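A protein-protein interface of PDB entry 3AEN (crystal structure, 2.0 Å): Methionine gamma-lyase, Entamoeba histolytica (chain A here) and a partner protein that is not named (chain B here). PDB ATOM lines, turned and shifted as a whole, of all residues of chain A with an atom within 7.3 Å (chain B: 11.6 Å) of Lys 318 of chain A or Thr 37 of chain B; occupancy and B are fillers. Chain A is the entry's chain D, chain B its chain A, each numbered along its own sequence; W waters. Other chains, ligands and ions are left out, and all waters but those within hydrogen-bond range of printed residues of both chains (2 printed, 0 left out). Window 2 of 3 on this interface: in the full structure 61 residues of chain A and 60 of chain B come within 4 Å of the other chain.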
ATOM      1  N   MET A 311      23.794  33.542 -16.140  1.00  0.00           N
ATOM      2  CA  MET A 311      22.599  33.731 -16.979  1.00  0.00           C
ATOM      3  C   MET A 311      21.455  34.198 -16.098  1.00  0.00           C
ATOM      4  O   MET A 311      21.572  34.176 -14.869  1.00  0.00           O
ATOM      5  CB  MET A 311      22.165  32.423 -17.647  1.00  0.00           C
ATOM      6  CG  MET A 311      23.248  31.681 -18.413  1.00  0.00           C
ATOM      7  SD  MET A 311      23.737  32.474 -19.954  1.00  0.00           S
ATOM      8  CE  MET A 311      22.193  32.954 -20.730  1.00  0.00           C
ATOM      9  N   SER A 313      18.499  32.756 -15.816  1.00  0.00           N
ATOM     10  CA  SER A 313      17.760  31.629 -15.248  1.00  0.00           C
ATOM     11  C   SER A 313      18.389  30.290 -15.634  1.00  0.00           C
ATOM     12  O   SER A 313      19.289  30.237 -16.485  1.00  0.00           O
ATOM     13  CB  SER A 313      16.289  31.658 -15.675  1.00  0.00           C
ATOM     14  OG  SER A 313      16.164  31.317 -17.036  1.00  0.00           O
ATOM     15  N   PHE A 314      17.914  29.205 -15.024  1.00  0.00           N
ATOM     16  CA  PHE A 314      18.382  27.884 -15.437  1.00  0.00           C
ATOM     17  C   PHE A 314      18.009  27.577 -16.892  1.00  0.00           C
ATOM     18  O   PHE A 314      18.858  27.113 -17.657  1.00  0.00           O
ATOM     19  CB  PHE A 314      17.893  26.762 -14.514  1.00  0.00           C
ATOM     20  CG  PHE A 314      18.261  25.393 -15.006  1.00  0.00           C
ATOM     21  CD1 PHE A 314      17.298  24.545 -15.547  1.00  0.00           C
ATOM     22  CD2 PHE A 314      19.589  24.965 -14.972  1.00  0.00           C
ATOM     23  CE1 PHE A 314      17.661  23.266 -16.034  1.00  0.00           C
ATOM     24  CE2 PHE A 314      19.960  23.701 -15.452  1.00  0.00           C
ATOM     25  CZ  PHE A 314      18.990  22.851 -15.983  1.00  0.00           C
ATOM     26  N   GLU A 315      16.746  27.829 -17.260  1.00  0.00           N
ATOM     27  CA  GLU A 315      16.250  27.559 -18.618  1.00  0.00           C
ATOM     28  C   GLU A 315      17.103  28.249 -19.682  1.00  0.00           C
ATOM     29  O   GLU A 315      17.396  27.662 -20.724  1.00  0.00           O
ATOM     30  CB  GLU A 315      14.768  27.951 -18.785  1.00  0.00           C
ATOM     31  CG  GLU A 315      13.749  27.058 -18.023  1.00  0.00           C
ATOM     32  CD  GLU A 315      14.003  25.538 -18.172  1.00  0.00           C
ATOM     33  OE1 GLU A 315      13.949  24.813 -17.145  1.00  0.00           O
ATOM     34  OE2 GLU A 315      14.256  25.065 -19.307  1.00  0.00           O
ATOM     35  N   ALA A 316      17.498  29.489 -19.400  1.00  0.00           N
ATOM     36  CA  ALA A 316      18.381  30.252 -20.272  1.00  0.00           C
ATOM     37  C   ALA A 316      19.787  29.624 -20.371  1.00  0.00           C
ATOM     38  O   ALA A 316      20.360  29.559 -21.459  1.00  0.00           O
ATOM     39  CB  ALA A 316      18.447  31.714 -19.820  1.00  0.00           C
ATOM     40  N   ALA A 317      20.333  29.148 -19.252  1.00  0.00           N
ATOM     41  CA  ALA A 317      21.638  28.468 -19.260  1.00  0.00           C
ATOM     42  C   ALA A 317      21.597  27.187 -20.094  1.00  0.00           C
ATOM     43  O   ALA A 317      22.467  26.948 -20.932  1.00  0.00           O
ATOM     44  CB  ALA A 317      22.104  28.170 -17.845  1.00  0.00           C
ATOM     45  N   LYS A 318      20.570  26.377 -19.856  1.00  0.00           N
ATOM     46  CA  LYS A 318      20.342  25.139 -20.588  1.00  0.00           C
ATOM     47  C   LYS A 318      20.208  25.400 -22.090  1.00  0.00           C
ATOM     48  O   LYS A 318      20.741  24.650 -22.908  1.00  0.00           O
ATOM     49  CB  LYS A 318      19.091  24.436 -20.043  1.00  0.00           C
ATOM     50  CG  LYS A 318      18.727  23.156 -20.760  1.00  0.00           C
ATOM     51  CD  LYS A 318      17.350  22.662 -20.347  1.00  0.00           C
ATOM     52  CE  LYS A 318      16.838  21.591 -21.306  1.00  0.00           C
ATOM     53  NZ  LYS A 318      15.394  21.341 -21.097  1.00  0.00           N
ATOM     54  N   LYS A 319      19.503  26.469 -22.447  1.00  0.00           N
ATOM     55  CA  LYS A 319      19.332  26.818 -23.855  1.00  0.00           C
ATOM     56  C   LYS A 319      20.653  27.220 -24.529  1.00  0.00           C
ATOM     57  O   LYS A 319      20.911  26.824 -25.672  1.00  0.00           O
ATOM     58  CB  LYS A 319      18.264  27.891 -24.025  1.00  0.00           C
ATOM     59  CG  LYS A 319      17.602  27.884 -25.394  1.00  0.00           C
ATOM     60  CD  LYS A 319      16.308  28.676 -25.369  1.00  0.00           C
ATOM     61  CE  LYS A 319      16.018  29.328 -26.725  1.00  0.00           C
ATOM     62  NZ  LYS A 319      15.051  30.458 -26.535  1.00  0.00           N
ATOM     63  N   LEU A 320      21.491  27.984 -23.823  1.00  0.00           N
ATOM     64  CA  LEU A 320      22.795  28.339 -24.361  1.00  0.00           C
ATOM     65  C   LEU A 320      23.677  27.103 -24.545  1.00  0.00           C
ATOM     66  O   LEU A 320      24.185  26.869 -25.636  1.00  0.00           O
ATOM     67  CB  LEU A 320      23.517  29.394 -23.504  1.00  0.00           C
ATOM     68  CG  LEU A 320      25.015  29.555 -23.870  1.00  0.00           C
ATOM     69  CD1 LEU A 320      25.223  30.140 -25.277  1.00  0.00           C
ATOM     70  CD2 LEU A 320      25.752  30.387 -22.833  1.00  0.00           C
ATOM     71  N   MET A 321      23.833  26.321 -23.476  1.00  0.00           N
ATOM     72  CA  MET A 321      24.701  25.142 -23.460  1.00  0.00           C
ATOM     73  C   MET A 321      24.312  24.066 -24.462  1.00  0.00           C
ATOM     74  O   MET A 321      25.155  23.268 -24.860  1.00  0.00           O
ATOM     75  CB  MET A 321      24.750  24.523 -22.065  1.00  0.00           C
ATOM     76  CG  MET A 321      25.589  25.283 -21.066  1.00  0.00           C
ATOM     77  SD  MET A 321      25.575  24.488 -19.446  1.00  0.00           S
ATOM     78  CE  MET A 321      23.875  24.731 -18.915  1.00  0.00           C
ATOM     79  N   GLU A 322      23.046  24.045 -24.868  1.00  0.00           N
ATOM     80  CA  GLU A 322      22.547  22.977 -25.737  1.00  0.00           C
ATOM     81  C   GLU A 322      22.370  23.349 -27.214  1.00  0.00           C
ATOM     82  O   GLU A 322      21.982  22.493 -28.014  1.00  0.00           O
ATOM     83  CB  GLU A 322      21.241  22.400 -25.178  1.00  0.00           C
ATOM     84  CG  GLU A 322      21.444  21.496 -23.975  1.00  0.00           C
ATOM     85  CD  GLU A 322      20.142  21.109 -23.286  1.00  0.00           C
ATOM     86  OE1 GLU A 322      20.199  20.633 -22.134  1.00  0.00           O
ATOM     87  OE2 GLU A 322      19.058  21.283 -23.880  1.00  0.00           O
ATOM     88  N   HIS A 323      22.641  24.606 -27.578  1.00  0.00           N
ATOM     89  CA  HIS A 323      22.570  25.041 -28.992  1.00  0.00           C
ATOM     90  C   HIS A 323      23.884  25.606 -29.530  1.00  0.00           C
ATOM     91  O   HIS A 323      23.894  26.490 -30.394  1.00  0.00           O
ATOM     92  CB  HIS A 323      21.404  26.007 -29.212  1.00  0.00           C
ATOM     93  CG  HIS A 323      20.073  25.367 -28.999  1.00  0.00           C
ATOM     94  ND1 HIS A 323      19.440  25.359 -27.775  1.00  0.00           N
ATOM     95  CD2 HIS A 323      19.281  24.659 -29.838  1.00  0.00           C
ATOM     96  CE1 HIS A 323      18.300  24.699 -27.875  1.00  0.00           C
ATOM     97  NE2 HIS A 323      18.177  24.267 -29.118  1.00  0.00           N
ATOM     98  N   LEU A 329      29.901  20.507 -25.032  1.00  0.00           N
ATOM     99  CA  LEU A 329      29.434  20.322 -23.661  1.00  0.00           C
ATOM    100  C   LEU A 329      30.155  19.102 -23.048  1.00  0.00           C
ATOM    101  O   LEU A 329      29.958  17.968 -23.483  1.00  0.00           O
ATOM    102  CB  LEU A 329      27.916  20.160 -23.635  1.00  0.00           C
ATOM    103  CG  LEU A 329      27.199  20.022 -22.285  1.00  0.00           C
ATOM    104  CD1 LEU A 329      27.293  21.263 -21.398  1.00  0.00           C
ATOM    105  CD2 LEU A 329      25.734  19.652 -22.509  1.00  0.00           C
ATOM    106  N   GLU A 341      30.351  23.873 -19.528  1.00  0.00           N
ATOM    107  CA  GLU A 341      29.966  23.020 -18.418  1.00  0.00           C
ATOM    108  C   GLU A 341      28.976  23.739 -17.488  1.00  0.00           C
ATOM    109  O   GLU A 341      28.971  24.971 -17.418  1.00  0.00           O
ATOM    110  CB  GLU A 341      31.243  22.697 -17.662  1.00  0.00           C
ATOM    111  CG  GLU A 341      31.160  21.615 -16.720  1.00  0.00           C
ATOM    112  CD  GLU A 341      31.121  22.094 -15.273  1.00  0.00           C
ATOM    113  OE1 GLU A 341      31.841  23.038 -14.858  1.00  0.00           O
ATOM    114  OE2 GLU A 341      30.372  21.459 -14.528  1.00  0.00           O
ATOM    115  N   HIS A 342      28.166  22.963 -16.762  1.00  0.00           N
ATOM    116  CA  HIS A 342      27.220  23.500 -15.764  1.00  0.00           C
ATOM    117  C   HIS A 342      27.661  23.028 -14.385  1.00  0.00           C
ATOM    118  O   HIS A 342      27.314  21.920 -13.980  1.00  0.00           O
ATOM    119  CB  HIS A 342      25.790  23.015 -16.058  1.00  0.00           C
ATOM    120  CG  HIS A 342      24.735  23.660 -15.212  1.00  0.00           C
ATOM    121  ND1 HIS A 342      24.087  22.995 -14.190  1.00  0.00           N
ATOM    122  CD2 HIS A 342      24.195  24.903 -15.255  1.00  0.00           C
ATOM    123  CE1 HIS A 342      23.202  23.802 -13.635  1.00  0.00           C
ATOM    124  NE2 HIS A 342      23.254  24.968 -14.258  1.00  0.00           N
ATOM    125  N   SER A 345      25.358  21.182 -11.479  1.00  0.00           N
ATOM    126  CA  SER A 345      24.877  19.817 -11.736  1.00  0.00           C
ATOM    127  C   SER A 345      25.957  18.888 -12.297  1.00  0.00           C
ATOM    128  O   SER A 345      25.700  17.709 -12.539  1.00  0.00           O
ATOM    129  CB  SER A 345      23.641  19.837 -12.654  1.00  0.00           C
ATOM    130  OG  SER A 345      24.004  20.124 -13.992  1.00  0.00           O
ATOM    131  N   MET A 346      27.167  19.412 -12.491  1.00  0.00           N
ATOM    132  CA  MET A 346      28.284  18.610 -13.000  1.00  0.00           C
ATOM    133  C   MET A 346      29.525  18.652 -12.072  1.00  0.00           C
ATOM    134  O   MET A 346      29.570  17.917 -11.077  1.00  0.00           O
ATOM    135  CB  MET A 346      28.613  18.976 -14.460  1.00  0.00           C
ATOM    136  CG  MET A 346      27.416  18.940 -15.423  1.00  0.00           C
ATOM    137  SD  MET A 346      27.836  19.491 -17.092  1.00  0.00           S
ATOM    138  CE  MET A 346      26.210  19.609 -17.848  1.00  0.00           C
ATOM    139  N   PRO A 363      22.307  27.452 -10.007  1.00  0.00           N
ATOM    140  CA  PRO A 363      22.004  26.814 -11.293  1.00  0.00           C
ATOM    141  C   PRO A 363      22.067  27.766 -12.512  1.00  0.00           C
ATOM    142  O   PRO A 363      21.987  27.299 -13.659  1.00  0.00           O
ATOM    143  CB  PRO A 363      20.578  26.276 -11.090  1.00  0.00           C
ATOM    144  CG  PRO A 363      20.358  26.283  -9.601  1.00  0.00           C
ATOM    145  CD  PRO A 363      21.138  27.447  -9.106  1.00  0.00           C
ATOM    146  N   VAL A 366      27.211  29.213 -15.846  1.00  0.00           N
ATOM    147  CA  VAL A 366      27.803  28.372 -16.888  1.00  0.00           C
ATOM    148  C   VAL A 366      29.318  28.625 -16.881  1.00  0.00           C
ATOM    149  O   VAL A 366      29.749  29.782 -16.818  1.00  0.00           O
ATOM    150  CB  VAL A 366      27.225  28.741 -18.272  1.00  0.00           C
ATOM    151  CG1 VAL A 366      27.855  27.903 -19.393  1.00  0.00           C
ATOM    152  CG2 VAL A 366      25.722  28.574 -18.276  1.00  0.00           C
ATOM    153  N   PHE B  32      34.775  13.295 -21.915  1.00  0.00           N
ATOM    154  CA  PHE B  32      33.723  12.724 -22.763  1.00  0.00           C
ATOM    155  C   PHE B  32      32.630  13.762 -22.981  1.00  0.00           C
ATOM    156  O   PHE B  32      32.430  14.646 -22.135  1.00  0.00           O
ATOM    157  CB  PHE B  32      33.110  11.482 -22.095  1.00  0.00           C
ATOM    158  CG  PHE B  32      34.023  10.303 -22.076  1.00  0.00           C
ATOM    159  CD1 PHE B  32      34.952  10.146 -21.050  1.00  0.00           C
ATOM    160  CD2 PHE B  32      33.972   9.355 -23.096  1.00  0.00           C
ATOM    161  CE1 PHE B  32      35.836   9.076 -21.047  1.00  0.00           C
ATOM    162  CE2 PHE B  32      34.831   8.256 -23.093  1.00  0.00           C
ATOM    163  CZ  PHE B  32      35.769   8.125 -22.069  1.00  0.00           C
ATOM    164  N   CYS B  33      31.905  13.635 -24.090  1.00  0.00           N
ATOM    165  CA  CYS B  33      30.895  14.616 -24.492  1.00  0.00           C
ATOM    166  C   CYS B  33      29.519  14.263 -23.960  1.00  0.00           C
ATOM    167  O   CYS B  33      29.166  13.081 -23.860  1.00  0.00           O
ATOM    168  CB  CYS B  33      30.849  14.733 -26.028  1.00  0.00           C
ATOM    169  SG  CYS B  33      32.488  15.019 -26.747  1.00  0.00           S
ATOM    170  N   PHE B  34      28.741  15.294 -23.633  1.00  0.00           N
ATOM    171  CA  PHE B  34      27.370  15.110 -23.192  1.00  0.00           C
ATOM    172  C   PHE B  34      26.422  15.458 -24.327  1.00  0.00           C
ATOM    173  O   PHE B  34      26.660  16.408 -25.080  1.00  0.00           O
ATOM    174  CB  PHE B  34      27.055  15.988 -21.968  1.00  0.00           C
ATOM    175  CG  PHE B  34      27.844  15.635 -20.715  1.00  0.00           C
ATOM    176  CD1 PHE B  34      28.205  14.316 -20.426  1.00  0.00           C
ATOM    177  CD2 PHE B  34      28.168  16.629 -19.793  1.00  0.00           C
ATOM    178  CE1 PHE B  34      28.915  13.998 -19.254  1.00  0.00           C
ATOM    179  CE2 PHE B  34      28.865  16.328 -18.619  1.00  0.00           C
ATOM    180  CZ  PHE B  34      29.245  14.996 -18.348  1.00  0.00           C
ATOM    181  N   ASP B  35      25.347  14.688 -24.450  1.00  0.00           N
ATOM    182  CA  ASP B  35      24.285  14.996 -25.411  1.00  0.00           C
ATOM    183  C   ASP B  35      23.448  16.222 -25.025  1.00  0.00           C
ATOM    184  O   ASP B  35      22.849  16.867 -25.886  1.00  0.00           O
ATOM    185  CB  ASP B  35      23.353  13.790 -25.581  1.00  0.00           C
ATOM    186  CG  ASP B  35      24.058  12.588 -26.187  1.00  0.00           C
ATOM    187  OD1 ASP B  35      24.921  12.761 -27.084  1.00  0.00           O
ATOM    188  OD2 ASP B  35      23.740  11.459 -25.768  1.00  0.00           O
ATOM    189  N   SER B  36      23.404  16.518 -23.727  1.00  0.00           N
ATOM    190  CA  SER B  36      22.527  17.542 -23.176  1.00  0.00           C
ATOM    191  C   SER B  36      22.894  17.754 -21.718  1.00  0.00           C
ATOM    192  O   SER B  36      23.585  16.913 -21.127  1.00  0.00           O
ATOM    193  CB  SER B  36      21.066  17.084 -23.264  1.00  0.00           C
ATOM    194  OG  SER B  36      20.814  16.017 -22.368  1.00  0.00           O
ATOM    195  N   THR B  37      22.414  18.854 -21.134  1.00  0.00           N
ATOM    196  CA  THR B  37      22.682  19.138 -19.727  1.00  0.00           C
ATOM    197  C   THR B  37      22.124  18.017 -18.836  1.00  0.00           C
ATOM    198  O   THR B  37      22.829  17.507 -17.953  1.00  0.00           O
ATOM    199  CB  THR B  37      22.123  20.519 -19.289  1.00  0.00           C
ATOM    200  OG1 THR B  37      20.720  20.558 -19.546  1.00  0.00           O
ATOM    201  CG2 THR B  37      22.770  21.631 -20.074  1.00  0.00           C
ATOM    202  N   GLN B  38      20.876  17.623 -19.106  1.00  0.00           N
ATOM    203  CA  GLN B  38      20.203  16.525 -18.403  1.00  0.00           C
ATOM    204  C   GLN B  38      20.974  15.201 -18.476  1.00  0.00           C
ATOM    205  O   GLN B  38      21.157  14.515 -17.458  1.00  0.00           O
ATOM    206  CB  GLN B  38      18.774  16.335 -18.935  1.00  0.00           C
ATOM    207  CG  GLN B  38      17.872  15.475 -18.044  1.00  0.00           C
ATOM    208  CD  GLN B  38      17.839  15.961 -16.599  1.00  0.00           C
ATOM    209  OE1 GLN B  38      17.187  16.954 -16.272  1.00  0.00           O
ATOM    210  NE2 GLN B  38      18.545  15.253 -15.726  1.00  0.00           N
ATOM    211  N   GLN B  39      21.435  14.844 -19.672  1.00  0.00           N
ATOM    212  CA  GLN B  39      22.145  13.579 -19.846  1.00  0.00           C
ATOM    213  C   GLN B  39      23.428  13.566 -19.011  1.00  0.00           C
ATOM    214  O   GLN B  39      23.730  12.566 -18.362  1.00  0.00           O
ATOM    215  CB  GLN B  39      22.402  13.293 -21.325  1.00  0.00           C
ATOM    216  CG  GLN B  39      23.001  11.906 -21.616  1.00  0.00           C
ATOM    217  CD  GLN B  39      24.517  11.941 -21.788  1.00  0.00           C
ATOM    218  OE1 GLN B  39      25.098  12.988 -22.102  1.00  0.00           O
ATOM    219  NE2 GLN B  39      25.166  10.789 -21.591  1.00  0.00           N
ATOM    220  N   GLY B  40      24.146  14.693 -19.004  1.00  0.00           N
ATOM    221  CA  GLY B  40      25.333  14.900 -18.169  1.00  0.00           C
ATOM    222  C   GLY B  40      25.050  14.947 -16.670  1.00  0.00           C
ATOM    223  O   GLY B  40      25.764  14.308 -15.880  1.00  0.00           O
ATOM    224  N   ALA B  41      24.021  15.701 -16.276  1.00  0.00           N
ATOM    225  CA  ALA B  41      23.568  15.746 -14.879  1.00  0.00           C
ATOM    226  C   ALA B  41      23.278  14.343 -14.332  1.00  0.00           C
ATOM    227  O   ALA B  41      23.763  13.977 -13.251  1.00  0.00           O
ATOM    228  CB  ALA B  41      22.321  16.639 -14.736  1.00  0.00           C
ATOM    229  N   ASP B  42      22.493  13.577 -15.094  1.00  0.00           N
ATOM    230  CA  ASP B  42      22.115  12.200 -14.771  1.00  0.00           C
ATOM    231  C   ASP B  42      23.328  11.280 -14.544  1.00  0.00           C
ATOM    232  O   ASP B  42      23.367  10.535 -13.547  1.00  0.00           O
ATOM    233  CB  ASP B  42      21.221  11.629 -15.869  1.00  0.00           C
ATOM    234  CG  ASP B  42      19.772  12.101 -15.763  1.00  0.00           C
ATOM    235  OD1 ASP B  42      19.396  12.789 -14.799  1.00  0.00           O
ATOM    236  OD2 ASP B  42      18.984  11.770 -16.660  1.00  0.00           O
ATOM    237  N   LEU B  43      24.317  11.346 -15.442  1.00  0.00           N
ATOM    238  CA  LEU B  43      25.529  10.534 -15.295  1.00  0.00           C
ATOM    239  C   LEU B  43      26.238  10.861 -13.991  1.00  0.00           C
ATOM    240  O   LEU B  43      26.716   9.968 -13.318  1.00  0.00           O
ATOM    241  CB  LEU B  43      26.483  10.683 -16.488  1.00  0.00           C
ATOM    242  CG  LEU B  43      26.092   9.894 -17.744  1.00  0.00           C
ATOM    243  CD1 LEU B  43      27.047  10.176 -18.918  1.00  0.00           C
ATOM    244  CD2 LEU B  43      25.994   8.382 -17.482  1.00  0.00           C
ATOM    245  N   PHE B  44      26.260  12.142 -13.617  1.00  0.00           N
ATOM    246  CA  PHE B  44      26.874  12.548 -12.349  1.00  0.00           C
ATOM    247  C   PHE B  44      26.153  11.987 -11.124  1.00  0.00           C
ATOM    248  O   PHE B  44      26.787  11.774 -10.090  1.00  0.00           O
ATOM    249  CB  PHE B  44      27.029  14.077 -12.252  1.00  0.00           C
ATOM    250  CG  PHE B  44      28.355  14.576 -12.768  1.00  0.00           C
ATOM    251  CD1 PHE B  44      28.478  15.052 -14.060  1.00  0.00           C
ATOM    252  CD2 PHE B  44      29.494  14.534 -11.956  1.00  0.00           C
ATOM    253  CE1 PHE B  44      29.715  15.501 -14.534  1.00  0.00           C
ATOM    254  CE2 PHE B  44      30.723  14.983 -12.415  1.00  0.00           C
ATOM    255  CZ  PHE B  44      30.841  15.465 -13.700  1.00  0.00           C
ATOM    256  N   MET B  45      24.851  11.722 -11.270  1.00  0.00           N
ATOM    257  CA  MET B  45      24.020  11.131 -10.220  1.00  0.00           C
ATOM    258  C   MET B  45      24.022   9.601 -10.276  1.00  0.00           C
ATOM    259  O   MET B  45      23.368   8.955  -9.469  1.00  0.00           O
ATOM    260  CB  MET B  45      22.573  11.640 -10.326  1.00  0.00           C
ATOM    261  CG  MET B  45      22.354  13.096  -9.929  1.00  0.00           C
ATOM    262  SD  MET B  45      20.693  13.620 -10.466  1.00  0.00           S
ATOM    263  CE  MET B  45      20.756  15.431 -10.301  1.00  0.00           C
ATOM    264  N   GLY B  46      24.747   9.020 -11.234  1.00  0.00           N
ATOM    265  CA  GLY B  46      24.754   7.571 -11.403  1.00  0.00           C
ATOM    266  C   GLY B  46      23.586   7.028 -12.211  1.00  0.00           C
ATOM    267  O   GLY B  46      23.364   5.832 -12.247  1.00  0.00           O
ATOM    268  N   LYS B  47      22.858   7.916 -12.875  1.00  0.00           N
ATOM    269  CA  LYS B  47      21.694   7.560 -13.665  1.00  0.00           C
ATOM    270  C   LYS B  47      22.076   7.488 -15.154  1.00  0.00           C
ATOM    271  O   LYS B  47      22.690   8.415 -15.699  1.00  0.00           O
ATOM    272  CB  LYS B  47      20.580   8.593 -13.423  1.00  0.00           C
ATOM    273  CG  LYS B  47      19.267   8.277 -14.139  1.00  0.00           C
ATOM    274  CD  LYS B  47      18.177   9.301 -13.850  1.00  0.00           C
ATOM    275  CE  LYS B  47      16.863   8.868 -14.488  1.00  0.00           C
ATOM    276  NZ  LYS B  47      15.811   9.915 -14.371  1.00  0.00           N
ATOM    277  N   GLY B  48      21.715   6.382 -15.804  1.00  0.00           N
ATOM    278  CA  GLY B  48      21.994   6.188 -17.219  1.00  0.00           C
ATOM    279  C   GLY B  48      23.340   5.537 -17.477  1.00  0.00           C
ATOM    280  O   GLY B  48      24.145   5.353 -16.561  1.00  0.00           O
ATOM    281  N   HIS B  51      29.889   7.735 -20.070  1.00  0.00           N
ATOM    282  CA  HIS B  51      31.141   8.158 -19.447  1.00  0.00           C
ATOM    283  C   HIS B  51      31.202   9.682 -19.267  1.00  0.00           C
ATOM    284  O   HIS B  51      30.500  10.433 -19.956  1.00  0.00           O
ATOM    285  CB  HIS B  51      32.326   7.627 -20.260  1.00  0.00           C
ATOM    286  CG  HIS B  51      32.448   6.137 -20.210  1.00  0.00           C
ATOM    287  ND1 HIS B  51      31.717   5.301 -21.030  1.00  0.00           N
ATOM    288  CD2 HIS B  51      33.175   5.330 -19.397  1.00  0.00           C
ATOM    289  CE1 HIS B  51      31.996   4.043 -20.730  1.00  0.00           C
ATOM    290  NE2 HIS B  51      32.883   4.034 -19.747  1.00  0.00           N
ATOM    291  N   ILE B  52      32.038  10.115 -18.323  1.00  0.00           N
ATOM    292  CA  ILE B  52      32.161  11.513 -17.935  1.00  0.00           C
ATOM    293  C   ILE B  52      33.605  12.002 -18.139  1.00  0.00           C
ATOM    294  O   ILE B  52      33.842  13.005 -18.808  1.00  0.00           O
ATOM    295  CB  ILE B  52      31.822  11.724 -16.422  1.00  0.00           C
ATOM    296  CG1 ILE B  52      30.388  11.298 -16.090  1.00  0.00           C
ATOM    297  CG2 ILE B  52      32.088  13.176 -16.034  1.00  0.00           C
ATOM    298  CD1 ILE B  52      29.976  11.590 -14.654  1.00  0.00           C
HETATM  299  O   HOH W   1      18.588  18.586 -20.995  1.00  0.00           O
HETATM  300  O   HOH W   2      24.097  16.009 -11.251  1.00  0.00           O
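Lys 318 of chain A touches just one residue of chain B: Thr 37 (3.5 Å). No residue of chain B comes within 4 Å of Phe 314 of chain A. No residue of chain B comes within 4 Å of Glu 315 of chain A. No residue of chain B comes within 4 Å of Leu 320 of chain A. Met 321 of chain A touches just one residue of chain B: Thr 37. Glu 322 of chain A touches two residues of chain B. Of the printed residues of chain B, Ser 345 of chain A touches Ala 41 (3.7 Å) and Phe 44 (3.9 Å). Printed residues of chain A within 4 Å of Cys 33 of chain B: Leu 329 (3.6 Å). Of the printed residues of chain A, Phe 44 of chain B touches Ser 345 (3.9 Å) and Met 346 (3.4 Å). Pro 363 of chain A touches none of the printed residues of chain B. Met 45 of chain B touches none of the printed residues of chain A. The nearest printed residue of chain B that does not touch Met 346 of chain A is Ala 41 of chain B (4.7 Å).
Of the 19 printed residues of chain B, 6 touch a printed residue of chain A. Printed residues of chain B that touch a printed residue of chain A: Cys 33, Phe 34, Ser 36, Thr 37, Ala 41 and Phe 44. Hydrophobic or aromatic side chains of chain B that line the printed part of chain A: Phe 34, Ala 41 and Phe 44. Of the 19 printed residues of chain A, 6 touch a printed residue of chain B. Among the printed residues, no Asp or Glu carboxylate lies within 4 Å of a Lys or Arg side-chain nitrogen of the other chain.
Lys 318 of chain A touches Thr 37 of chain B. Met 321 of chain A touches Thr 37 of chain B. Ser 36 of chain B touches Glu 322 of chain A (CB to OE1, 3.8 Å). O of Leu 329 of chain A touches CA of Cys 33 of chain B, at 3.6 Å. Leu 329 of chain A touches Ser 36 of chain B (CD2 to C, 3.5 Å). Ser 345 of chain A touches Ala 41 of chain B (O to CA, 3.7 Å). Ser 345 of chain A touches Phe 44 of chain B (O to CB, 3.9 Å). Phe 34 of chain B touches Met 346 of chain A. O of Thr 37 of chain B touches CE of Met 346 of chain A, at 3.98 Å. Phe 44 of chain B touches Met 346 of chain A.
OG of Ser 36 of chain B is in hydrogen-bond range of N of Gln 39 of chain B, at 3.0 Å. A ring nitrogen (ND1) of His 342 of chain A is in hydrogen-bond range of the side-chain hydroxyl (OG) of Ser 345 of chain A, at 2.9 Å. SD of Met 346 of chain A sits at hydrogen-bond distance from N of His 342 of chain A.
N of Phe 34 of chain B is in hydrogen-bond range of O of Leu 329 of chain A (2.9 Å). OE1 of Glu 322 of chain A is in hydrogen-bond range of OG1 of Thr 37 of chain B (2.6 Å).
Water W2 lies within hydrogen-bond range of O of Ser 345 of chain A and O of Ala 41 of chain B. Water W1 lies within hydrogen-bond range of OE1 of Glu 322 of chain A (2.8 Å), N of Gln 38 of chain B (3.1 Å) and OG1 of Thr 37 of chain B (3.2 Å).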
